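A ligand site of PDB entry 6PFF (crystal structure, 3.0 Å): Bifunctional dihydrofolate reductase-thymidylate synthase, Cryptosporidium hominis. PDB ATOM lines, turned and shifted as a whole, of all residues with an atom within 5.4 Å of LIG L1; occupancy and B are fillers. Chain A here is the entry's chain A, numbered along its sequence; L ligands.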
ATOM      1  N   VAL A   9      -6.501  26.134  -2.927  1.00  0.00           N
ATOM      2  CA  VAL A   9      -6.482  26.422  -1.496  1.00  0.00           C
ATOM      3  C   VAL A   9      -7.640  25.660  -0.876  1.00  0.00           C
ATOM      4  O   VAL A   9      -8.803  25.899  -1.235  1.00  0.00           O
ATOM      5  CB  VAL A   9      -6.601  27.931  -1.198  1.00  0.00           C
ATOM      6  CG1 VAL A   9      -6.321  28.193   0.270  1.00  0.00           C
ATOM      7  CG2 VAL A   9      -5.650  28.724  -2.075  1.00  0.00           C
ATOM      8  N   VAL A  10      -7.341  24.756   0.054  1.00  0.00           N
ATOM      9  CA  VAL A  10      -8.375  23.885   0.602  1.00  0.00           C
ATOM     10  C   VAL A  10      -8.056  23.566   2.057  1.00  0.00           C
ATOM     11  O   VAL A  10      -6.894  23.528   2.464  1.00  0.00           O
ATOM     12  CB  VAL A  10      -8.539  22.609  -0.245  1.00  0.00           C
ATOM     13  CG1 VAL A  10      -7.271  21.748  -0.173  1.00  0.00           C
ATOM     14  CG2 VAL A  10      -9.761  21.808   0.199  1.00  0.00           C
ATOM     15  N   ALA A  11      -9.115  23.353   2.835  1.00  0.00           N
ATOM     16  CA  ALA A  11      -9.010  22.857   4.198  1.00  0.00           C
ATOM     17  C   ALA A  11      -9.818  21.573   4.279  1.00  0.00           C
ATOM     18  O   ALA A  11     -11.038  21.592   4.123  1.00  0.00           O
ATOM     19  CB  ALA A  11      -9.519  23.888   5.215  1.00  0.00           C
ATOM     20  N   LEU A  25     -19.039  24.762   6.478  1.00  0.00           N
ATOM     21  CA  LEU A  25     -17.823  24.068   6.881  1.00  0.00           C
ATOM     22  C   LEU A  25     -18.120  23.177   8.081  1.00  0.00           C
ATOM     23  O   LEU A  25     -18.954  23.513   8.932  1.00  0.00           O
ATOM     24  CB  LEU A  25     -16.739  25.071   7.253  1.00  0.00           C
ATOM     25  CG  LEU A  25     -16.087  25.883   6.132  1.00  0.00           C
ATOM     26  CD1 LEU A  25     -15.105  26.861   6.725  1.00  0.00           C
ATOM     27  CD2 LEU A  25     -15.410  24.973   5.127  1.00  0.00           C
ATOM     28  N   SER A  30     -10.752  30.057  13.106  1.00  0.00           N
ATOM     29  CA  SER A  30     -10.546  31.443  12.677  1.00  0.00           C
ATOM     30  C   SER A  30      -9.186  31.616  12.002  1.00  0.00           C
ATOM     31  O   SER A  30      -9.083  32.325  10.987  1.00  0.00           O
ATOM     32  CB  SER A  30     -10.663  32.374  13.875  1.00  0.00           C
ATOM     33  OG  SER A  30     -10.597  33.735  13.467  1.00  0.00           O
ATOM     34  N   ASP A  32      -7.572  29.597  10.248  1.00  0.00           N
ATOM     35  CA  ASP A  32      -7.580  29.048   8.895  1.00  0.00           C
ATOM     36  C   ASP A  32      -8.182  30.050   7.903  1.00  0.00           C
ATOM     37  O   ASP A  32      -7.703  30.181   6.772  1.00  0.00           O
ATOM     38  CB  ASP A  32      -8.344  27.734   8.865  1.00  0.00           C
ATOM     39  CG  ASP A  32      -8.506  27.185   7.461  1.00  0.00           C
ATOM     40  OD1 ASP A  32      -7.474  26.935   6.798  1.00  0.00           O
ATOM     41  OD2 ASP A  32      -9.662  27.021   7.024  1.00  0.00           O
ATOM     42  N   LEU A  33      -9.246  30.751   8.305  1.00  0.00           N
ATOM     43  CA  LEU A  33      -9.770  31.810   7.456  1.00  0.00           C
ATOM     44  C   LEU A  33      -8.759  32.936   7.295  1.00  0.00           C
ATOM     45  O   LEU A  33      -8.599  33.499   6.196  1.00  0.00           O
ATOM     46  CB  LEU A  33     -11.088  32.349   8.013  1.00  0.00           C
ATOM     47  CG  LEU A  33     -12.276  31.399   7.939  1.00  0.00           C
ATOM     48  CD1 LEU A  33     -13.553  32.110   8.373  1.00  0.00           C
ATOM     49  CD2 LEU A  33     -12.421  30.825   6.535  1.00  0.00           C
ATOM     50  N   LYS A  34      -8.041  33.271   8.375  1.00  0.00           N
ATOM     51  CA  LYS A  34      -7.001  34.291   8.261  1.00  0.00           C
ATOM     52  C   LYS A  34      -5.902  33.836   7.297  1.00  0.00           C
ATOM     53  O   LYS A  34      -5.371  34.640   6.524  1.00  0.00           O
ATOM     54  CB  LYS A  34      -6.421  34.607   9.639  1.00  0.00           C
ATOM     55  N   PHE A  35      -5.565  32.539   7.321  1.00  0.00           N
ATOM     56  CA  PHE A  35      -4.576  32.003   6.384  1.00  0.00           C
ATOM     57  C   PHE A  35      -5.075  32.097   4.956  1.00  0.00           C
ATOM     58  O   PHE A  35      -4.327  32.481   4.049  1.00  0.00           O
ATOM     59  CB  PHE A  35      -4.242  30.555   6.737  1.00  0.00           C
ATOM     60  CG  PHE A  35      -3.333  29.883   5.744  1.00  0.00           C
ATOM     61  CD1 PHE A  35      -1.980  30.178   5.709  1.00  0.00           C
ATOM     62  CD2 PHE A  35      -3.838  28.964   4.829  1.00  0.00           C
ATOM     63  CE1 PHE A  35      -1.143  29.569   4.801  1.00  0.00           C
ATOM     64  CE2 PHE A  35      -3.000  28.347   3.913  1.00  0.00           C
ATOM     65  CZ  PHE A  35      -1.652  28.650   3.899  1.00  0.00           C
ATOM     66  N   PHE A  36      -6.339  31.722   4.719  1.00  0.00           N
ATOM     67  CA  PHE A  36      -6.912  31.871   3.383  1.00  0.00           C
ATOM     68  C   PHE A  36      -6.800  33.310   2.911  1.00  0.00           C
ATOM     69  O   PHE A  36      -6.380  33.575   1.774  1.00  0.00           O
ATOM     70  CB  PHE A  36      -8.373  31.409   3.391  1.00  0.00           C
ATOM     71  CG  PHE A  36      -9.077  31.589   2.076  1.00  0.00           C
ATOM     72  CD1 PHE A  36      -9.105  30.554   1.149  1.00  0.00           C
ATOM     73  CD2 PHE A  36      -9.709  32.782   1.765  1.00  0.00           C
ATOM     74  CE1 PHE A  36      -9.743  30.715  -0.060  1.00  0.00           C
ATOM     75  CE2 PHE A  36     -10.346  32.943   0.556  1.00  0.00           C
ATOM     76  CZ  PHE A  36     -10.370  31.907  -0.354  1.00  0.00           C
ATOM     77  N   SER A  37      -7.154  34.263   3.782  1.00  0.00           N
ATOM     78  CA  SER A  37      -7.094  35.669   3.414  1.00  0.00           C
ATOM     79  C   SER A  37      -5.671  36.088   3.060  1.00  0.00           C
ATOM     80  O   SER A  37      -5.446  36.732   2.030  1.00  0.00           O
ATOM     81  CB  SER A  37      -7.653  36.529   4.551  1.00  0.00           C
ATOM     82  OG  SER A  37      -7.476  37.913   4.268  1.00  0.00           O
ATOM     83  N   THR A  40      -4.428  34.391  -0.278  1.00  0.00           N
ATOM     84  CA  THR A  40      -5.058  34.845  -1.509  1.00  0.00           C
ATOM     85  C   THR A  40      -4.794  36.314  -1.813  1.00  0.00           C
ATOM     86  O   THR A  40      -4.954  36.741  -2.959  1.00  0.00           O
ATOM     87  CB  THR A  40      -6.567  34.593  -1.470  1.00  0.00           C
ATOM     88  OG1 THR A  40      -7.135  35.203  -0.314  1.00  0.00           O
ATOM     89  CG2 THR A  40      -6.842  33.090  -1.430  1.00  0.00           C
ATOM     90  N   ASN A  41      -4.399  37.096  -0.807  1.00  0.00           N
ATOM     91  CA  ASN A  41      -3.991  38.481  -1.013  1.00  0.00           C
ATOM     92  C   ASN A  41      -2.520  38.626  -1.372  1.00  0.00           C
ATOM     93  O   ASN A  41      -2.097  39.700  -1.816  1.00  0.00           O
ATOM     94  CB  ASN A  41      -4.274  39.313   0.241  1.00  0.00           C
ATOM     95  CG  ASN A  41      -5.710  39.787   0.329  1.00  0.00           C
ATOM     96  OD1 ASN A  41      -6.349  40.063  -0.692  1.00  0.00           O
ATOM     97  ND2 ASN A  41      -6.239  39.880   1.536  1.00  0.00           N
ATOM     98  N   MET A  54     -14.344  29.895  -7.738  1.00  0.00           N
ATOM     99  CA  MET A  54     -15.157  29.085  -6.836  1.00  0.00           C
ATOM    100  C   MET A  54     -16.465  28.704  -7.506  1.00  0.00           C
ATOM    101  O   MET A  54     -16.936  29.395  -8.421  1.00  0.00           O
ATOM    102  CB  MET A  54     -15.413  29.832  -5.516  1.00  0.00           C
ATOM    103  CG  MET A  54     -16.148  31.158  -5.675  1.00  0.00           C
ATOM    104  SD  MET A  54     -16.399  32.012  -4.099  1.00  0.00           S
ATOM    105  CE  MET A  54     -14.710  32.338  -3.597  1.00  0.00           C
ATOM    106  N   THR A  58     -20.377  27.260  -3.280  1.00  0.00           N
ATOM    107  CA  THR A  58     -19.393  27.957  -2.468  1.00  0.00           C
ATOM    108  C   THR A  58     -19.654  29.456  -2.449  1.00  0.00           C
ATOM    109  O   THR A  58     -19.566  30.113  -1.397  1.00  0.00           O
ATOM    110  CB  THR A  58     -17.987  27.661  -2.996  1.00  0.00           C
ATOM    111  OG1 THR A  58     -17.639  26.304  -2.665  1.00  0.00           O
ATOM    112  CG2 THR A  58     -16.959  28.595  -2.407  1.00  0.00           C
ATOM    113  N   ILE A  62     -20.491  31.919   1.138  1.00  0.00           N
ATOM    114  CA  ILE A  62     -19.860  33.127   1.623  1.00  0.00           C
ATOM    115  C   ILE A  62     -20.797  34.323   1.545  1.00  0.00           C
ATOM    116  O   ILE A  62     -20.357  35.473   1.588  1.00  0.00           O
ATOM    117  CB  ILE A  62     -18.533  33.399   0.909  1.00  0.00           C
ATOM    118  CG1 ILE A  62     -18.762  33.688  -0.574  1.00  0.00           C
ATOM    119  CG2 ILE A  62     -17.596  32.209   1.053  1.00  0.00           C
ATOM    120  CD1 ILE A  62     -17.486  34.027  -1.324  1.00  0.00           C
ATOM    121  N   LEU A  67     -14.952  39.606  -1.756  1.00  0.00           N
ATOM    122  CA  LEU A  67     -13.805  39.584  -0.863  1.00  0.00           C
ATOM    123  C   LEU A  67     -12.905  40.773  -1.198  1.00  0.00           C
ATOM    124  O   LEU A  67     -12.598  41.000  -2.370  1.00  0.00           O
ATOM    125  CB  LEU A  67     -13.033  38.267  -0.990  1.00  0.00           C
ATOM    126  CG  LEU A  67     -13.733  37.019  -0.458  1.00  0.00           C
ATOM    127  CD1 LEU A  67     -13.026  35.750  -0.901  1.00  0.00           C
ATOM    128  CD2 LEU A  67     -13.829  37.076   1.061  1.00  0.00           C
ATOM    129  N   ARG A  70      -9.735  41.465  -3.948  1.00  0.00           N
ATOM    130  CA  ARG A  70      -9.635  40.299  -4.817  1.00  0.00           C
ATOM    131  C   ARG A  70     -10.839  40.238  -5.747  1.00  0.00           C
ATOM    132  O   ARG A  70     -11.882  40.849  -5.483  1.00  0.00           O
ATOM    133  CB  ARG A  70      -9.509  39.017  -3.991  1.00  0.00           C
ATOM    134  CG  ARG A  70      -8.220  38.940  -3.196  1.00  0.00           C
ATOM    135  CD  ARG A  70      -8.328  37.959  -2.032  1.00  0.00           C
ATOM    136  NE  ARG A  70      -9.191  38.507  -0.987  1.00  0.00           N
ATOM    137  CZ  ARG A  70      -9.431  37.909   0.170  1.00  0.00           C
ATOM    138  NH1 ARG A  70      -8.901  36.727   0.439  1.00  0.00           N
ATOM    139  NH2 ARG A  70     -10.224  38.495   1.065  1.00  0.00           N
ATOM    140  N   CYS A 113     -10.439  27.705  -5.182  1.00  0.00           N
ATOM    141  CA  CYS A 113     -10.829  27.471  -3.805  1.00  0.00           C
ATOM    142  C   CYS A 113     -12.308  27.112  -3.690  1.00  0.00           C
ATOM    143  O   CYS A 113     -12.880  27.213  -2.603  1.00  0.00           O
ATOM    144  CB  CYS A 113     -10.498  28.688  -2.944  1.00  0.00           C
ATOM    145  SG  CYS A 113     -10.785  30.272  -3.767  1.00  0.00           S
ATOM    146  N   TYR A 119     -12.699  21.551  -7.522  1.00  0.00           N
ATOM    147  CA  TYR A 119     -11.409  20.922  -7.270  1.00  0.00           C
ATOM    148  C   TYR A 119     -11.194  19.714  -8.181  1.00  0.00           C
ATOM    149  O   TYR A 119     -10.134  19.553  -8.787  1.00  0.00           O
ATOM    150  CB  TYR A 119     -11.319  20.471  -5.809  1.00  0.00           C
ATOM    151  CG  TYR A 119     -11.214  21.578  -4.786  1.00  0.00           C
ATOM    152  CD1 TYR A 119     -10.479  22.725  -5.039  1.00  0.00           C
ATOM    153  CD2 TYR A 119     -11.862  21.463  -3.562  1.00  0.00           C
ATOM    154  CE1 TYR A 119     -10.388  23.734  -4.089  1.00  0.00           C
ATOM    155  CE2 TYR A 119     -11.783  22.460  -2.615  1.00  0.00           C
ATOM    156  CZ  TYR A 119     -11.036  23.590  -2.879  1.00  0.00           C
ATOM    157  OH  TYR A 119     -10.961  24.580  -1.926  1.00  0.00           O
ATOM    158  N   TYR A 132      -2.357  24.399  -1.385  1.00  0.00           N
ATOM    159  CA  TYR A 132      -2.233  24.833   0.006  1.00  0.00           C
ATOM    160  C   TYR A 132      -3.305  24.084   0.788  1.00  0.00           C
ATOM    161  O   TYR A 132      -4.487  24.448   0.767  1.00  0.00           O
ATOM    162  CB  TYR A 132      -2.410  26.352   0.134  1.00  0.00           C
ATOM    163  CG  TYR A 132      -1.343  27.174  -0.534  1.00  0.00           C
ATOM    164  CD1 TYR A 132      -0.211  27.586   0.164  1.00  0.00           C
ATOM    165  CD2 TYR A 132      -1.458  27.557  -1.865  1.00  0.00           C
ATOM    166  CE1 TYR A 132       0.771  28.344  -0.447  1.00  0.00           C
ATOM    167  CE2 TYR A 132      -0.485  28.317  -2.480  1.00  0.00           C
ATOM    168  CZ  TYR A 132       0.628  28.704  -1.771  1.00  0.00           C
ATOM    169  OH  TYR A 132       1.601  29.463  -2.385  1.00  0.00           O
ATOM    170  N   THR A 134      -4.871  22.612   4.300  1.00  0.00           N
ATOM    171  CA  THR A 134      -4.986  22.731   5.749  1.00  0.00           C
ATOM    172  C   THR A 134      -5.598  21.439   6.254  1.00  0.00           C
ATOM    173  O   THR A 134      -6.804  21.204   6.080  1.00  0.00           O
ATOM    174  CB  THR A 134      -5.812  23.949   6.140  1.00  0.00           C
ATOM    175  OG1 THR A 134      -5.260  25.116   5.525  1.00  0.00           O
ATOM    176  CG2 THR A 134      -5.821  24.120   7.651  1.00  0.00           C
HETATM  177  N1  LIG L   1      -9.966  27.232   4.318  1.00  0.00           N
HETATM  178  C1  LIG L   1      -8.911  26.972   3.521  1.00  0.00           C
HETATM  179  N2  LIG L   1      -7.649  26.635   4.136  1.00  0.00           N
HETATM  180  N3  LIG L   1      -8.987  27.024   2.186  1.00  0.00           N
HETATM  181  C2  LIG L   1     -10.161  27.345   1.587  1.00  0.00           C
HETATM  182  N4  LIG L   1     -10.280  27.406   0.162  1.00  0.00           N
HETATM  183  C3  LIG L   1     -11.288  27.612   2.381  1.00  0.00           C
HETATM  184  N5  LIG L   1     -12.483  27.922   1.806  1.00  0.00           N
HETATM  185  C4  LIG L   1     -13.540  28.169   2.603  1.00  0.00           C
HETATM  186  C5  LIG L   1     -13.460  28.130   3.998  1.00  0.00           C
HETATM  187  N6  LIG L   1     -12.261  27.811   4.553  1.00  0.00           N
HETATM  188  C6  LIG L   1     -11.174  27.545   3.753  1.00  0.00           C
HETATM  189  C7  LIG L   1     -14.828  28.525   1.919  1.00  0.00           C
HETATM  190  N7  LIG L   1     -14.649  29.773   1.219  1.00  0.00           N
HETATM  191  C8  LIG L   1     -14.594  29.816  -0.222  1.00  0.00           C
HETATM  192  C9  LIG L   1     -14.084  33.316   3.428  1.00  0.00           C
HETATM  193  C10 LIG L   1     -14.936  32.341   3.923  1.00  0.00           C
HETATM  194  C11 LIG L   1     -15.132  31.171   3.194  1.00  0.00           C
HETATM  195  C12 LIG L   1     -14.459  30.987   1.989  1.00  0.00           C
HETATM  196  C13 LIG L   1     -13.598  31.968   1.503  1.00  0.00           C
HETATM  197  C14 LIG L   1     -13.414  33.126   2.229  1.00  0.00           C
HETATM  198  C15 LIG L   1     -13.828  34.605   4.170  1.00  0.00           C
HETATM  199  O1  LIG L   1     -14.685  35.088   4.885  1.00  0.00           O
HETATM  200  N8  LIG L   1     -12.538  35.235   3.998  1.00  0.00           N
HETATM  201  C16 LIG L   1     -12.166  36.467   4.656  1.00  0.00           C
HETATM  202  C17 LIG L   1     -11.079  37.048   3.836  1.00  0.00           C
HETATM  203  O2  LIG L   1     -10.520  36.331   2.960  1.00  0.00           O
HETATM  204  O3  LIG L   1     -10.717  38.247   4.007  1.00  0.00           O
HETATM  205  C18 LIG L   1     -11.620  36.099   5.988  1.00  0.00           C
HETATM  206  C19 LIG L   1     -11.292  37.159   6.992  1.00  0.00           C
HETATM  207  C20 LIG L   1     -10.643  36.672   8.246  1.00  0.00           C
HETATM  208  O4  LIG L   1      -9.604  37.239   8.643  1.00  0.00           O
HETATM  209  O5  LIG L   1     -11.307  35.950   9.044  1.00  0.00           O
HETATM  210  P1  LG2 L   2     -19.548  23.860  -5.381  1.00  0.00           P
HETATM  211  O1  LG2 L   2     -18.497  23.068  -6.133  1.00  0.00           O
HETATM  212  O2  LG2 L   2     -18.896  24.919  -4.537  1.00  0.00           O
HETATM  213  O3  LG2 L   2     -20.457  24.572  -6.384  1.00  0.00           O
HETATM  214  C1  LG2 L   2     -21.139  23.842  -7.370  1.00  0.00           C
HETATM  215  C2  LG2 L   2     -21.789  24.630  -8.432  1.00  0.00           C
HETATM  216  O4  LG2 L   2     -20.794  25.157  -9.295  1.00  0.00           O
HETATM  217  C3  LG2 L   2     -22.648  23.817  -9.293  1.00  0.00           C
HETATM  218  O5  LG2 L   2     -23.930  23.724  -8.768  1.00  0.00           O
HETATM  219  C4  LG2 L   2     -22.633  24.564 -10.526  1.00  0.00           C
HETATM  220  O6  LG2 L   2     -23.429  25.707 -10.419  1.00  0.00           O
HETATM  221  C5  LG2 L   2     -21.262  25.014 -10.623  1.00  0.00           C
HETATM  222  N1  LG2 L   2     -20.462  24.081 -11.347  1.00  0.00           N
HETATM  223  C6  LG2 L   2     -19.668  23.125 -10.823  1.00  0.00           C
HETATM  224  N2  LG2 L   2     -19.073  22.437 -11.816  1.00  0.00           N
HETATM  225  C7  LG2 L   2     -19.488  22.968 -13.009  1.00  0.00           C
HETATM  226  C8  LG2 L   2     -19.218  22.685 -14.374  1.00  0.00           C
HETATM  227  N3  LG2 L   2     -18.281  21.582 -14.712  1.00  0.00           N
HETATM  228  N4  LG2 L   2     -19.805  23.425 -15.361  1.00  0.00           N
HETATM  229  C9  LG2 L   2     -20.655  24.426 -15.017  1.00  0.00           C
HETATM  230  N5  LG2 L   2     -20.943  24.726 -13.749  1.00  0.00           N
HETATM  231  C10 LG2 L   2     -20.367  24.009 -12.715  1.00  0.00           C
HETATM  232  O7  LG2 L   2     -20.422  22.909  -4.438  1.00  0.00           O
HETATM  233  P2  LG2 L   2     -19.796  21.774  -3.520  1.00  0.00           P
HETATM  234  O8  LG2 L   2     -20.892  20.900  -2.888  1.00  0.00           O
HETATM  235  O9  LG2 L   2     -18.913  20.883  -4.367  1.00  0.00           O
HETATM  236  O10 LG2 L   2     -18.923  22.483  -2.350  1.00  0.00           O
HETATM  237  C11 LG2 L   2     -19.550  23.241  -1.350  1.00  0.00           C
HETATM  238  C12 LG2 L   2     -19.364  22.802   0.023  1.00  0.00           C
HETATM  239  O11 LG2 L   2     -17.966  22.657   0.283  1.00  0.00           O
HETATM  240  C13 LG2 L   2     -19.843  23.813   0.976  1.00  0.00           C
HETATM  241  O12 LG2 L   2     -20.224  23.189   2.155  1.00  0.00           O
HETATM  242  C14 LG2 L   2     -18.686  24.617   1.220  1.00  0.00           C
HETATM  243  O13 LG2 L   2     -18.793  25.258   2.454  1.00  0.00           O
HETATM  244  C15 LG2 L   2     -17.605  23.602   1.223  1.00  0.00           C
HETATM  245  N6  LG2 L   2     -16.337  24.222   0.924  1.00  0.00           N
HETATM  246  C16 LG2 L   2     -15.272  23.913   1.688  1.00  0.00           C
HETATM  247  C17 LG2 L   2     -14.020  24.485   1.439  1.00  0.00           C
HETATM  248  C18 LG2 L   2     -12.837  24.119   2.327  1.00  0.00           C
HETATM  249  O14 LG2 L   2     -11.714  24.549   2.036  1.00  0.00           O
HETATM  250  N7  LG2 L   2     -12.989  23.289   3.482  1.00  0.00           N
HETATM  251  C19 LG2 L   2     -13.864  25.394   0.378  1.00  0.00           C
HETATM  252  C20 LG2 L   2     -14.991  25.692  -0.398  1.00  0.00           C
HETATM  253  C21 LG2 L   2     -16.227  25.103  -0.113  1.00  0.00           C
HETATM  254  P3  LG2 L   2     -24.806  25.799 -11.140  1.00  0.00           P
HETATM  255  O15 LG2 L   2     -25.720  24.691 -10.567  1.00  0.00           O
HETATM  256  O16 LG2 L   2     -25.384  27.131 -10.881  1.00  0.00           O
HETATM  257  O17 LG2 L   2     -24.648  25.630 -12.616  1.00  0.00           O
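The backbone carbonyl oxygen of Val 9 lies within hydrogen-bond range of a nitrogen (N4) of LIG L1 (2.5 Å).
The side-chain carboxylate (OD1) of Asp 32 lies within hydrogen-bond range of a nitrogen (N2) of LIG L1 (2.7 Å).
NH2 of Arg 70 lies within salt-bridge range of O2 of LIG L1 (2.9 Å).
OG1 of Thr 134 sits at hydrogen-bond distance from N2 of LIG L1 (3.2 Å).
The side-chain hydroxyl (OG) of Ser 37 is in hydrogen-bond range of an oxygen (O3) of LIG L1.
The backbone NH of Thr 58 is in hydrogen-bond range of an oxygen (O2) of LG2 L2, at 3.0 Å.
OG1 of Thr 58 sits at hydrogen-bond distance from O2 of LG2 L2 (2.6 Å).
An oxygen (O14) of LG2 L2 is in hydrogen-bond range of the backbone NH of Ala 11.
The backbone carbonyl oxygen (O) of Ala 11 is in hydrogen-bond range of a nitrogen (N7) of LG2 L2.
O of Val 9 lies within hydrogen-bond range of OH of Tyr 119 (2.6 Å).
OG1 of Thr 134 is in hydrogen-bond range of OD1 of Asp 32 (3.1 Å).
The guanidinium group of Arg 70 is in hydrogen-bond range of the side-chain hydroxyl of Thr 40.
NE of Arg 70 sits close to OD1 of Asn 41 (3.3 Å).
O of Val 10 is in hydrogen-bond range of N of Thr 134 (2.9 Å).
O of Ser 37 sits at hydrogen-bond distance from OG1 of Thr 40 (3.3 Å).
O of Phe 36 sits at hydrogen-bond distance from OG1 of Thr 40, at 2.8 Å.
The backbone carbonyl oxygen of Cys 113 sits at hydrogen-bond distance from the side-chain hydroxyl of Tyr 119 (3.3 Å).
Merely in contact with LIG L1: Phe 36 (3.4 Å), Cys 113 (3.4 Å), Ile 62 (3.4 Å), Leu 25 (3.4 Å), Thr 58 (3.4 Å), Ala 11 (3.5 Å), Val 10 (3.5 Å), Tyr 119 (3.6 Å), Leu 33 (3.6 Å), Leu 67 (3.7 Å) and Lys 34 (3.95 Å).
Hydrophobic or aromatic side chains within 4 Å of LIG L1: Val 9, Ala 11, Leu 25, Leu 33, Phe 36, Ile 62 and Leu 67.
Within 4 Å of LIG L1: Val 9, Val 10, Ala 11, Leu 25, Asp 32, Leu 33, Lys 34, Phe 36, Ser 37, Thr 58, Ile 62, Leu 67, Arg 70, Cys 113, Tyr 119 and Thr 134.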
